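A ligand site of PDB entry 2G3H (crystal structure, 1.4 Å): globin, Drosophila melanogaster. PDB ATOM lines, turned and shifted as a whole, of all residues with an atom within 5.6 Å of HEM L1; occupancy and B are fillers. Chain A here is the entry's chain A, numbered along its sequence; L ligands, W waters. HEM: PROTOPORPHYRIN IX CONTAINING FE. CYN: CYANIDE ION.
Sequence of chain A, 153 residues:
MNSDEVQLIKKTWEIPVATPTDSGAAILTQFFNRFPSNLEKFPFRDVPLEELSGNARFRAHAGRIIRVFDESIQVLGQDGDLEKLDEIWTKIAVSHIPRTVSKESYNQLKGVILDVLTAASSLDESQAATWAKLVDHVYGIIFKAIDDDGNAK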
ATOM      1  N   PHE A  31      15.502 -35.234  19.459  1.00  0.00           N
ATOM      2  CA  PHE A  31      16.138 -34.672  20.630  1.00  0.00           C
ATOM      3  C   PHE A  31      15.123 -34.431  21.743  1.00  0.00           C
ATOM      4  O   PHE A  31      15.353 -34.867  22.871  1.00  0.00           O
ATOM      5  CB  PHE A  31      16.855 -33.377  20.212  1.00  0.00           C
ATOM      6  CG  PHE A  31      17.674 -32.692  21.278  1.00  0.00           C
ATOM      7  CD1 PHE A  31      18.597 -33.383  22.066  1.00  0.00           C
ATOM      8  CD2 PHE A  31      17.621 -31.325  21.409  1.00  0.00           C
ATOM      9  CE1 PHE A  31      19.442 -32.693  23.004  1.00  0.00           C
ATOM     10  CE2 PHE A  31      18.462 -30.658  22.325  1.00  0.00           C
ATOM     11  CZ  PHE A  31      19.368 -31.364  23.104  1.00  0.00           C
ATOM     12  N   ASN A  38      15.851 -30.811  27.683  1.00  0.00           N
ATOM     13  CA  ASN A  38      16.424 -29.794  26.799  1.00  0.00           C
ATOM     14  C   ASN A  38      15.385 -28.851  26.223  1.00  0.00           C
ATOM     15  O   ASN A  38      15.679 -27.702  25.912  1.00  0.00           O
ATOM     16  CB  ASN A  38      17.164 -30.484  25.662  1.00  0.00           C
ATOM     17  CG  ASN A  38      18.326 -31.260  26.198  1.00  0.00           C
ATOM     18  OD1 ASN A  38      19.284 -30.657  26.704  1.00  0.00           O
ATOM     19  ND2 ASN A  38      18.261 -32.607  26.153  1.00  0.00           N
ATOM     20  N   LEU A  39      14.155 -29.314  26.082  1.00  0.00           N
ATOM     21  CA  LEU A  39      13.112 -28.435  25.555  1.00  0.00           C
ATOM     22  C   LEU A  39      12.876 -27.240  26.461  1.00  0.00           C
ATOM     23  O   LEU A  39      12.481 -26.169  25.984  1.00  0.00           O
ATOM     24  CB  LEU A  39      11.847 -29.254  25.307  1.00  0.00           C
ATOM     25  CG  LEU A  39      10.605 -28.584  24.729  1.00  0.00           C
ATOM     26  CD1 LEU A  39      10.869 -27.729  23.442  1.00  0.00           C
ATOM     27  CD2 LEU A  39       9.537 -29.653  24.497  1.00  0.00           C
ATOM     28  N   LYS A  41      14.987 -25.302  27.689  1.00  0.00           N
ATOM     29  CA  LYS A  41      15.899 -24.190  27.365  1.00  0.00           C
ATOM     30  C   LYS A  41      15.325 -23.299  26.281  1.00  0.00           C
ATOM     31  O   LYS A  41      15.772 -22.161  26.132  1.00  0.00           O
ATOM     32  CB  LYS A  41      17.267 -24.705  26.898  1.00  0.00           C
ATOM     33  CG  LYS A  41      18.032 -25.548  27.889  1.00  0.00           C
ATOM     34  CD  LYS A  41      18.546 -24.766  29.072  1.00  0.00           C
ATOM     35  CE  LYS A  41      19.667 -25.526  29.827  1.00  0.00           C
ATOM     36  NZ  LYS A  41      20.099 -24.735  31.005  1.00  0.00           N
ATOM     37  N   PHE A  42      14.328 -23.788  25.538  1.00  0.00           N
ATOM     38  CA  PHE A  42      13.852 -23.088  24.345  1.00  0.00           C
ATOM     39  C   PHE A  42      12.573 -22.298  24.624  1.00  0.00           C
ATOM     40  O   PHE A  42      11.777 -22.662  25.480  1.00  0.00           O
ATOM     41  CB  PHE A  42      13.529 -24.076  23.234  1.00  0.00           C
ATOM     42  CG  PHE A  42      14.695 -24.725  22.644  1.00  0.00           C
ATOM     43  CD1 PHE A  42      15.222 -24.243  21.480  1.00  0.00           C
ATOM     44  CD2 PHE A  42      15.288 -25.820  23.230  1.00  0.00           C
ATOM     45  CE1 PHE A  42      16.358 -24.814  20.918  1.00  0.00           C
ATOM     46  CE2 PHE A  42      16.422 -26.406  22.641  1.00  0.00           C
ATOM     47  CZ  PHE A  42      16.926 -25.928  21.485  1.00  0.00           C
ATOM     48  N   PRO A  43      12.362 -21.186  23.898  1.00  0.00           N
ATOM     49  CA  PRO A  43      11.234 -20.328  24.191  1.00  0.00           C
ATOM     50  C   PRO A  43       9.876 -20.967  23.891  1.00  0.00           C
ATOM     51  O   PRO A  43       8.853 -20.517  24.391  1.00  0.00           O
ATOM     52  CB  PRO A  43      11.492 -19.085  23.343  1.00  0.00           C
ATOM     53  CG  PRO A  43      12.357 -19.541  22.221  1.00  0.00           C
ATOM     54  CD  PRO A  43      13.225 -20.639  22.829  1.00  0.00           C
ATOM     55  N   PHE A  44       9.896 -22.005  23.044  1.00  0.00           N
ATOM     56  CA  PHE A  44       8.706 -22.803  22.709  1.00  0.00           C
ATOM     57  C   PHE A  44       8.503 -23.986  23.657  1.00  0.00           C
ATOM     58  O   PHE A  44       7.730 -24.888  23.363  1.00  0.00           O
ATOM     59  CB  PHE A  44       8.691 -23.222  21.209  1.00  0.00           C
ATOM     60  CG  PHE A  44       9.996 -23.793  20.709  1.00  0.00           C
ATOM     61  CD1 PHE A  44      10.358 -25.090  21.024  1.00  0.00           C
ATOM     62  CD2 PHE A  44      10.817 -23.055  19.886  1.00  0.00           C
ATOM     63  CE1 PHE A  44      11.503 -25.642  20.538  1.00  0.00           C
ATOM     64  CE2 PHE A  44      11.999 -23.622  19.384  1.00  0.00           C
ATOM     65  CZ  PHE A  44      12.307 -24.931  19.703  1.00  0.00           C
ATOM     66  N   ARG A  57       8.247 -21.027  15.160  1.00  0.00           N
ATOM     67  CA  ARG A  57       9.571 -20.875  15.759  1.00  0.00           C
ATOM     68  C   ARG A  57      10.381 -22.172  15.591  1.00  0.00           C
ATOM     69  O   ARG A  57      11.570 -22.133  15.241  1.00  0.00           O
ATOM     70  CB  ARG A  57       9.482 -20.474  17.262  1.00  0.00           C
ATOM     71  CG  ARG A  57      10.880 -20.210  17.851  1.00  0.00           C
ATOM     72  CD  ARG A  57      11.551 -18.988  17.233  1.00  0.00           C
ATOM     73  NE  ARG A  57      12.703 -18.509  18.016  1.00  0.00           N
ATOM     74  CZ  ARG A  57      13.409 -17.431  17.725  1.00  0.00           C
ATOM     75  NH1 ARG A  57      13.089 -16.692  16.639  1.00  0.00           N
ATOM     76  NH2 ARG A  57      14.392 -17.068  18.529  1.00  0.00           N
ATOM     77  N   HIS A  61      13.741 -22.471  13.466  1.00  0.00           N
ATOM     78  CA  HIS A  61      14.934 -22.861  14.198  1.00  0.00           C
ATOM     79  C   HIS A  61      15.624 -24.114  13.569  1.00  0.00           C
ATOM     80  O   HIS A  61      16.847 -24.225  13.513  1.00  0.00           O
ATOM     81  CB  HIS A  61      14.610 -23.093  15.691  1.00  0.00           C
ATOM     82  CG  HIS A  61      15.840 -23.455  16.442  1.00  0.00           C
ATOM     83  ND1 HIS A  61      16.881 -22.569  16.631  1.00  0.00           N
ATOM     84  CD2 HIS A  61      16.259 -24.647  16.915  1.00  0.00           C
ATOM     85  CE1 HIS A  61      17.874 -23.216  17.207  1.00  0.00           C
ATOM     86  NE2 HIS A  61      17.509 -24.455  17.443  1.00  0.00           N
ATOM     87  N   ARG A  64      17.944 -22.962  11.089  1.00  0.00           N
ATOM     88  CA  ARG A  64      19.091 -22.328  11.656  1.00  0.00           C
ATOM     89  C   ARG A  64      20.193 -23.323  12.054  1.00  0.00           C
ATOM     90  O   ARG A  64      21.383 -23.060  11.833  1.00  0.00           O
ATOM     91  CB  ARG A  64      18.706 -21.468  12.854  1.00  0.00           C
ATOM     92  CG  ARG A  64      17.843 -20.298  12.518  1.00  0.00           C
ATOM     93  CD  ARG A  64      17.479 -19.445  13.750  1.00  0.00           C
ATOM     94  NE  ARG A  64      16.664 -18.319  13.285  1.00  0.00           N
ATOM     95  CZ  ARG A  64      15.350 -18.197  13.440  1.00  0.00           C
ATOM     96  NH1 ARG A  64      14.680 -18.977  14.248  1.00  0.00           N
ATOM     97  NH2 ARG A  64      14.683 -17.241  12.796  1.00  0.00           N
ATOM     98  N   ILE A  65      19.821 -24.445  12.638  1.00  0.00           N
ATOM     99  CA  ILE A  65      20.815 -25.408  13.045  1.00  0.00           C
ATOM    100  C   ILE A  65      21.430 -26.121  11.837  1.00  0.00           C
ATOM    101  O   ILE A  65      22.626 -26.398  11.850  1.00  0.00           O
ATOM    102  CB  ILE A  65      20.320 -26.384  14.204  1.00  0.00           C
ATOM    103  CG1 ILE A  65      21.519 -27.241  14.727  1.00  0.00           C
ATOM    104  CG2 ILE A  65      19.178 -27.248  13.743  1.00  0.00           C
ATOM    105  CD1 ILE A  65      21.226 -28.094  15.969  1.00  0.00           C
ATOM    106  N   VAL A  68      24.272 -23.895  10.198  1.00  0.00           N
ATOM    107  CA  VAL A  68      25.616 -24.010  10.819  1.00  0.00           C
ATOM    108  C   VAL A  68      26.382 -25.176  10.281  1.00  0.00           C
ATOM    109  O   VAL A  68      27.575 -25.092   9.989  1.00  0.00           O
ATOM    110  CB  VAL A  68      25.539 -24.196  12.394  1.00  0.00           C
ATOM    111  CG1 VAL A  68      26.979 -24.401  13.086  1.00  0.00           C
ATOM    112  CG2 VAL A  68      24.852 -23.081  12.986  1.00  0.00           C
ATOM    113  N   PHE A  69      25.704 -26.316  10.183  1.00  0.00           N
ATOM    114  CA  PHE A  69      26.381 -27.456   9.627  1.00  0.00           C
ATOM    115  C   PHE A  69      26.765 -27.253   8.181  1.00  0.00           C
ATOM    116  O   PHE A  69      27.829 -27.658   7.750  1.00  0.00           O
ATOM    117  CB  PHE A  69      25.526 -28.722   9.796  1.00  0.00           C
ATOM    118  CG  PHE A  69      25.649 -29.316  11.170  1.00  0.00           C
ATOM    119  CD1 PHE A  69      24.764 -28.988  12.183  1.00  0.00           C
ATOM    120  CD2 PHE A  69      26.674 -30.175  11.462  1.00  0.00           C
ATOM    121  CE1 PHE A  69      24.906 -29.531  13.447  1.00  0.00           C
ATOM    122  CE2 PHE A  69      26.810 -30.714  12.710  1.00  0.00           C
ATOM    123  CZ  PHE A  69      25.930 -30.374  13.705  1.00  0.00           C
ATOM    124  N   TRP A  89      32.508 -22.612  15.432  1.00  0.00           N
ATOM    125  CA  TRP A  89      32.054 -23.403  16.540  1.00  0.00           C
ATOM    126  C   TRP A  89      32.366 -22.761  17.894  1.00  0.00           C
ATOM    127  O   TRP A  89      31.652 -23.028  18.860  1.00  0.00           O
ATOM    128  CB  TRP A  89      32.559 -24.844  16.430  1.00  0.00           C
ATOM    129  CG  TRP A  89      31.849 -25.529  15.310  1.00  0.00           C
ATOM    130  CD1 TRP A  89      32.197 -25.531  14.003  1.00  0.00           C
ATOM    131  CD2 TRP A  89      30.603 -26.223  15.390  1.00  0.00           C
ATOM    132  NE1 TRP A  89      31.248 -26.182  13.251  1.00  0.00           N
ATOM    133  CE2 TRP A  89      30.260 -26.633  14.091  1.00  0.00           C
ATOM    134  CE3 TRP A  89      29.749 -26.533  16.450  1.00  0.00           C
ATOM    135  CZ2 TRP A  89      29.121 -27.372  13.831  1.00  0.00           C
ATOM    136  CZ3 TRP A  89      28.601 -27.264  16.183  1.00  0.00           C
ATOM    137  CH2 TRP A  89      28.310 -27.669  14.884  1.00  0.00           C
ATOM    138  N   LYS A  91      31.905 -19.571  18.137  1.00  0.00           N
ATOM    139  CA  LYS A  91      30.762 -18.652  18.147  1.00  0.00           C
ATOM    140  C   LYS A  91      29.520 -19.380  18.659  1.00  0.00           C
ATOM    141  O   LYS A  91      28.737 -18.825  19.443  1.00  0.00           O
ATOM    142  CB  LYS A  91      30.550 -18.041  16.761  1.00  0.00           C
ATOM    143  CG  LYS A  91      29.339 -17.164  16.536  1.00  0.00           C
ATOM    144  CD  LYS A  91      29.343 -16.513  15.152  1.00  0.00           C
ATOM    145  CE  LYS A  91      28.094 -15.639  14.953  1.00  0.00           C
ATOM    146  NZ  LYS A  91      27.935 -15.053  13.598  1.00  0.00           N
ATOM    147  N   ILE A  92      29.344 -20.634  18.260  1.00  0.00           N
ATOM    148  CA  ILE A  92      28.220 -21.454  18.802  1.00  0.00           C
ATOM    149  C   ILE A  92      28.377 -21.649  20.318  1.00  0.00           C
ATOM    150  O   ILE A  92      27.476 -21.368  21.100  1.00  0.00           O
ATOM    151  CB  ILE A  92      28.114 -22.858  18.055  1.00  0.00           C
ATOM    152  CG1 ILE A  92      27.645 -22.672  16.610  1.00  0.00           C
ATOM    153  CG2 ILE A  92      27.237 -23.877  18.839  1.00  0.00           C
ATOM    154  CD1 ILE A  92      26.342 -21.911  16.465  1.00  0.00           C
ATOM    155  N   SER A  95      27.529 -18.355  22.181  1.00  0.00           N
ATOM    156  CA  SER A  95      26.126 -17.935  22.226  1.00  0.00           C
ATOM    157  C   SER A  95      25.287 -18.848  23.125  1.00  0.00           C
ATOM    158  O   SER A  95      24.259 -18.418  23.648  1.00  0.00           O
ATOM    159  CB  SER A  95      25.517 -17.822  20.844  1.00  0.00           C
ATOM    160  OG  SER A  95      25.368 -19.106  20.277  1.00  0.00           O
ATOM    161  N   HIS A  96      25.735 -20.079  23.353  1.00  0.00           N
ATOM    162  CA  HIS A  96      25.014 -20.992  24.239  1.00  0.00           C
ATOM    163  C   HIS A  96      25.429 -20.903  25.706  1.00  0.00           C
ATOM    164  O   HIS A  96      24.687 -21.356  26.560  1.00  0.00           O
ATOM    165  CB  HIS A  96      25.146 -22.438  23.721  1.00  0.00           C
ATOM    166  CG  HIS A  96      24.397 -22.694  22.450  1.00  0.00           C
ATOM    167  ND1 HIS A  96      24.790 -22.212  21.211  1.00  0.00           N
ATOM    168  CD2 HIS A  96      23.258 -23.390  22.225  1.00  0.00           C
ATOM    169  CE1 HIS A  96      23.925 -22.623  20.290  1.00  0.00           C
ATOM    170  NE2 HIS A  96      23.002 -23.350  20.883  1.00  0.00           N
ATOM    171  N   ARG A  99      22.843 -19.813  28.133  1.00  0.00           N
ATOM    172  CA  ARG A  99      21.807 -20.820  28.223  1.00  0.00           C
ATOM    173  C   ARG A  99      22.203 -22.027  29.073  1.00  0.00           C
ATOM    174  O   ARG A  99      21.405 -22.943  29.239  1.00  0.00           O
ATOM    175  CB  ARG A  99      21.455 -21.313  26.815  1.00  0.00           C
ATOM    176  CG  ARG A  99      21.043 -20.217  25.847  1.00  0.00           C
ATOM    177  CD  ARG A  99      20.800 -20.749  24.458  1.00  0.00           C
ATOM    178  NE  ARG A  99      20.601 -19.598  23.579  1.00  0.00           N
ATOM    179  CZ  ARG A  99      21.200 -19.347  22.433  1.00  0.00           C
ATOM    180  NH1 ARG A  99      21.936 -20.274  21.837  1.00  0.00           N
ATOM    181  NH2 ARG A  99      21.028 -18.166  21.858  1.00  0.00           N
ATOM    182  N   VAL A 101      24.094 -24.645  28.662  1.00  0.00           N
ATOM    183  CA  VAL A 101      23.972 -25.924  27.967  1.00  0.00           C
ATOM    184  C   VAL A 101      25.154 -26.804  28.403  1.00  0.00           C
ATOM    185  O   VAL A 101      26.313 -26.508  28.069  1.00  0.00           O
ATOM    186  CB  VAL A 101      23.908 -25.743  26.451  1.00  0.00           C
ATOM    187  CG1 VAL A 101      23.897 -27.111  25.771  1.00  0.00           C
ATOM    188  CG2 VAL A 101      22.684 -24.882  26.051  1.00  0.00           C
ATOM    189  N   SER A 105      24.140 -32.388  27.879  1.00  0.00           N
ATOM    190  CA  SER A 105      23.112 -32.017  26.930  1.00  0.00           C
ATOM    191  C   SER A 105      23.647 -31.915  25.505  1.00  0.00           C
ATOM    192  O   SER A 105      22.985 -32.364  24.569  1.00  0.00           O
ATOM    193  CB  SER A 105      22.454 -30.693  27.367  1.00  0.00           C
ATOM    194  OG  SER A 105      21.775 -30.856  28.606  1.00  0.00           O
ATOM    195  N   TYR A 106      24.852 -31.354  25.324  1.00  0.00           N
ATOM    196  CA  TYR A 106      25.477 -31.384  23.994  1.00  0.00           C
ATOM    197  C   TYR A 106      25.643 -32.842  23.505  1.00  0.00           C
ATOM    198  O   TYR A 106      25.414 -33.153  22.348  1.00  0.00           O
ATOM    199  CB  TYR A 106      26.830 -30.686  24.052  1.00  0.00           C
ATOM    200  CG  TYR A 106      26.799 -29.181  23.840  1.00  0.00           C
ATOM    201  CD1 TYR A 106      26.407 -28.662  22.613  1.00  0.00           C
ATOM    202  CD2 TYR A 106      27.270 -28.309  24.800  1.00  0.00           C
ATOM    203  CE1 TYR A 106      26.455 -27.299  22.354  1.00  0.00           C
ATOM    204  CE2 TYR A 106      27.336 -26.948  24.583  1.00  0.00           C
ATOM    205  CZ  TYR A 106      26.939 -26.426  23.341  1.00  0.00           C
ATOM    206  OH  TYR A 106      27.018 -25.069  23.119  1.00  0.00           O
ATOM    207  N   LEU A 109      22.451 -34.384  22.177  1.00  0.00           N
ATOM    208  CA  LEU A 109      22.129 -33.937  20.822  1.00  0.00           C
ATOM    209  C   LEU A 109      23.087 -34.599  19.829  1.00  0.00           C
ATOM    210  O   LEU A 109      22.699 -34.907  18.719  1.00  0.00           O
ATOM    211  CB  LEU A 109      22.266 -32.420  20.713  1.00  0.00           C
ATOM    212  CG  LEU A 109      21.950 -31.820  19.362  1.00  0.00           C
ATOM    213  CD1 LEU A 109      20.499 -32.143  18.963  1.00  0.00           C
ATOM    214  CD2 LEU A 109      22.150 -30.310  19.360  1.00  0.00           C
ATOM    215  N   ILE A 113      21.987 -36.275  16.289  1.00  0.00           N
ATOM    216  CA  ILE A 113      22.400 -35.780  14.976  1.00  0.00           C
ATOM    217  C   ILE A 113      23.019 -36.918  14.184  1.00  0.00           C
ATOM    218  O   ILE A 113      22.699 -37.108  13.012  1.00  0.00           O
ATOM    219  CB  ILE A 113      23.438 -34.627  15.123  1.00  0.00           C
ATOM    220  CG1 ILE A 113      22.755 -33.399  15.732  1.00  0.00           C
ATOM    221  CG2 ILE A 113      24.084 -34.294  13.807  1.00  0.00           C
ATOM    222  CD1 ILE A 113      23.673 -32.270  16.196  1.00  0.00           C
ATOM    223  N   TYR A 139      32.890 -30.772  18.271  1.00  0.00           N
ATOM    224  CA  TYR A 139      32.541 -30.843  19.696  1.00  0.00           C
ATOM    225  C   TYR A 139      33.746 -30.509  20.523  1.00  0.00           C
ATOM    226  O   TYR A 139      33.621 -29.922  21.589  1.00  0.00           O
ATOM    227  CB  TYR A 139      31.984 -32.221  20.068  1.00  0.00           C
ATOM    228  CG  TYR A 139      30.449 -32.186  20.054  1.00  0.00           C
ATOM    229  CD1 TYR A 139      29.753 -31.813  18.924  1.00  0.00           C
ATOM    230  CD2 TYR A 139      29.718 -32.533  21.160  1.00  0.00           C
ATOM    231  CE1 TYR A 139      28.379 -31.753  18.893  1.00  0.00           C
ATOM    232  CE2 TYR A 139      28.334 -32.488  21.161  1.00  0.00           C
ATOM    233  CZ  TYR A 139      27.656 -32.079  20.038  1.00  0.00           C
ATOM    234  OH  TYR A 139      26.267 -32.009  20.021  1.00  0.00           O
ATOM    235  N   ILE A 142      33.753 -26.795  20.765  1.00  0.00           N
ATOM    236  CA  ILE A 142      32.776 -26.287  21.726  1.00  0.00           C
ATOM    237  C   ILE A 142      33.283 -26.515  23.147  1.00  0.00           C
ATOM    238  O   ILE A 142      33.244 -25.611  23.998  1.00  0.00           O
ATOM    239  CB  ILE A 142      31.409 -27.017  21.611  1.00  0.00           C
ATOM    240  CG1 ILE A 142      30.787 -26.764  20.225  1.00  0.00           C
ATOM    241  CG2 ILE A 142      30.467 -26.553  22.706  1.00  0.00           C
ATOM    242  CD1 ILE A 142      29.478 -27.464  20.013  1.00  0.00           C
HETATM  243  CHA HEM L   1      19.912 -21.435  19.366  1.00  0.00           C
HETATM  244  CHB HEM L   1      23.023 -24.145  16.847  1.00  0.00           C
HETATM  245  CHC HEM L   1      23.233 -27.232  20.546  1.00  0.00           C
HETATM  246  CHD HEM L   1      19.800 -24.758  22.896  1.00  0.00           C
HETATM  247  C1A HEM L   1      20.781 -21.875  18.417  1.00  0.00           C
HETATM  248  C2A HEM L   1      21.070 -21.179  17.162  1.00  0.00           C
HETATM  249  C3A HEM L   1      21.915 -21.947  16.465  1.00  0.00           C
HETATM  250  C4A HEM L   1      22.171 -23.151  17.224  1.00  0.00           C
HETATM  251  CMA HEM L   1      22.525 -21.660  15.059  1.00  0.00           C
HETATM  252  CAA HEM L   1      20.523 -19.790  16.760  1.00  0.00           C
HETATM  253  CBA HEM L   1      21.615 -18.729  16.798  1.00  0.00           C
HETATM  254  CGA HEM L   1      22.314 -18.530  18.101  1.00  0.00           C
HETATM  255  O1A HEM L   1      21.665 -18.340  19.134  1.00  0.00           O
HETATM  256  O2A HEM L   1      23.564 -18.517  18.087  1.00  0.00           O
HETATM  257  C1B HEM L   1      23.336 -25.196  17.686  1.00  0.00           C
HETATM  258  C2B HEM L   1      24.190 -26.227  17.345  1.00  0.00           C
HETATM  259  C3B HEM L   1      24.352 -27.068  18.375  1.00  0.00           C
HETATM  260  C4B HEM L   1      23.457 -26.593  19.379  1.00  0.00           C
HETATM  261  CMB HEM L   1      25.046 -26.272  16.007  1.00  0.00           C
HETATM  262  CAB HEM L   1      25.190 -28.338  18.548  1.00  0.00           C
HETATM  263  CBB HEM L   1      25.595 -29.043  17.527  1.00  0.00           C
HETATM  264  C1C HEM L   1      22.302 -26.848  21.463  1.00  0.00           C
HETATM  265  C2C HEM L   1      21.930 -27.627  22.612  1.00  0.00           C
HETATM  266  C3C HEM L   1      20.961 -26.964  23.275  1.00  0.00           C
HETATM  267  C4C HEM L   1      20.687 -25.731  22.542  1.00  0.00           C
HETATM  268  CMC HEM L   1      22.600 -28.961  22.979  1.00  0.00           C
HETATM  269  CAC HEM L   1      20.330 -27.464  24.588  1.00  0.00           C
HETATM  270  CBC HEM L   1      19.087 -27.255  24.892  1.00  0.00           C
HETATM  271  C1D HEM L   1      19.567 -23.639  22.136  1.00  0.00           C
HETATM  272  C2D HEM L   1      18.686 -22.666  22.468  1.00  0.00           C
HETATM  273  C3D HEM L   1      18.581 -21.673  21.375  1.00  0.00           C
HETATM  274  C4D HEM L   1      19.570 -22.122  20.479  1.00  0.00           C
HETATM  275  CMD HEM L   1      17.669 -22.646  23.641  1.00  0.00           C
HETATM  276  CAD HEM L   1      17.663 -20.449  21.304  1.00  0.00           C
HETATM  277  CBD HEM L   1      16.508 -20.903  20.420  1.00  0.00           C
HETATM  278  CGD HEM L   1      15.465 -19.878  20.069  1.00  0.00           C
HETATM  279  O1D HEM L   1      15.488 -18.754  20.648  1.00  0.00           O
HETATM  280  O2D HEM L   1      14.533 -20.245  19.271  1.00  0.00           O
HETATM  281  NA  HEM L   1      21.481 -23.079  18.449  1.00  0.00           N
HETATM  282  NB  HEM L   1      22.846 -25.400  18.921  1.00  0.00           N
HETATM  283  NC  HEM L   1      21.515 -25.713  21.411  1.00  0.00           N
HETATM  284  ND  HEM L   1      20.156 -23.328  20.950  1.00  0.00           N
HETATM  285 FE   HEM L   1      21.491 -24.391  19.937  1.00  0.00          FE
HETATM  286  C   CYN L   2      20.001 -25.529  19.069  1.00  0.00           C
HETATM  287  N   CYN L   2      19.207 -26.194  18.576  1.00  0.00           N
HETATM  288  O   HOH W   1      17.435 -17.099  21.336  1.00  0.00           O
HETATM  289  O   HOH W   2      15.934 -19.980  16.795  1.00  0.00           O
HETATM  290  O   HOH W   3      19.086 -17.636  19.204  1.00  0.00           O
HETATM  291  O   HOH W   4      24.638 -15.746  18.443  1.00  0.00           O
HETATM  292  O   HOH W   5      24.992 -17.609  16.060  1.00  0.00           O
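FE of HEM L1 is bound by NE2 of His 96, 2.1 Å away.
The guanidinium group (NH2) of Arg 99 lies within salt-bridge range of an oxygen (O1A) of HEM L1 (2.8 Å).
An oxygen (O2D) of HEM L1 lies within salt-bridge range of the guanidinium group (NE) of Arg 57 (2.8 Å).
The side-chain hydroxyl of Ser 95 lies within hydrogen-bond range of an oxygen (O2A) of HEM L1, 2.9 Å away.
A ring nitrogen (NE2) of His 61 is in hydrogen-bond range of a nitrogen (N) of CYN L2 (2.7 Å).
A ring nitrogen (NE2) of His 96 lies close to the guanidinium group (NH1) of Arg 99.
The side-chain hydroxyl (OG) of Ser 95 sits at hydrogen-bond distance from a ring nitrogen (ND1) of His 96, at 3.3 Å.
A ring nitrogen (ND1) of His 96 lies within hydrogen-bond range of the backbone carbonyl oxygen (O) of Ile 92, 2.8 Å away.
O of Ser 95 sits close to NH1 of Arg 99 (3.5 Å).
The backbone carbonyl oxygen of Arg 99 lies within hydrogen-bond range of the side-chain amino group of Lys 41 (2.8 Å).
OG of Ser 95 is in hydrogen-bond range of O of Lys 91.
The side-chain amide oxygen (OD1) of Asn 38 sits at hydrogen-bond distance from the side-chain hydroxyl (OG) of Ser 105 (3.1 Å).
O of Tyr 106 sits at hydrogen-bond distance from OH of Tyr 139, 2.7 Å away.
Asn 38 touches HEM L1.
Lys 41 touches HEM L1 (O to CMD, 3.2 Å).
Phe 42 touches HEM L1.
CG of Pro 43 touches O1D of HEM L1 (3.6 Å).
His 61 touches HEM L1 (CE1 to C1A, 3.4 Å).
Arg 64 touches HEM L1.
Ile 65 touches HEM L1.
CG2 of Val 68 touches CMA of HEM L1 (3.4 Å).
Trp 89 touches HEM L1 (CZ3 to CMB, 3.7 Å).
Val 101 touches HEM L1 (CG1 to CMC, 3.6 Å).
Ser 105 touches HEM L1 (O to CMC, 3.8 Å).
CE1 of Tyr 106 touches CHC of HEM L1, at 3.7 Å.
Leu 109 touches HEM L1 (CD2 to CHC, 3.5 Å).
Ile 113 touches HEM L1.
OH of Tyr 139 touches CBB of HEM L1, at 3.9 Å.
Hydrophobic or aromatic side chains that line HEM L1: Phe 42, Pro 43, His 61, Ile 65, Val 68, Trp 89, His 96, Val 101, Tyr 106, Leu 109 and Ile 113.
Of the 26 residues printed, 19 come within 4 Å of HEM L1.
The nearest printed residue that does not touch HEM L1 is Ile 92 (4.02 Å).
Water W3 lies within hydrogen-bond range of an oxygen (O1A) of HEM L1 and the guanidinium group of Arg 99.
Water W2 lies within hydrogen-bond range of ND1 of His 61, O2D of HEM L1 and NH1 of Arg 64.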
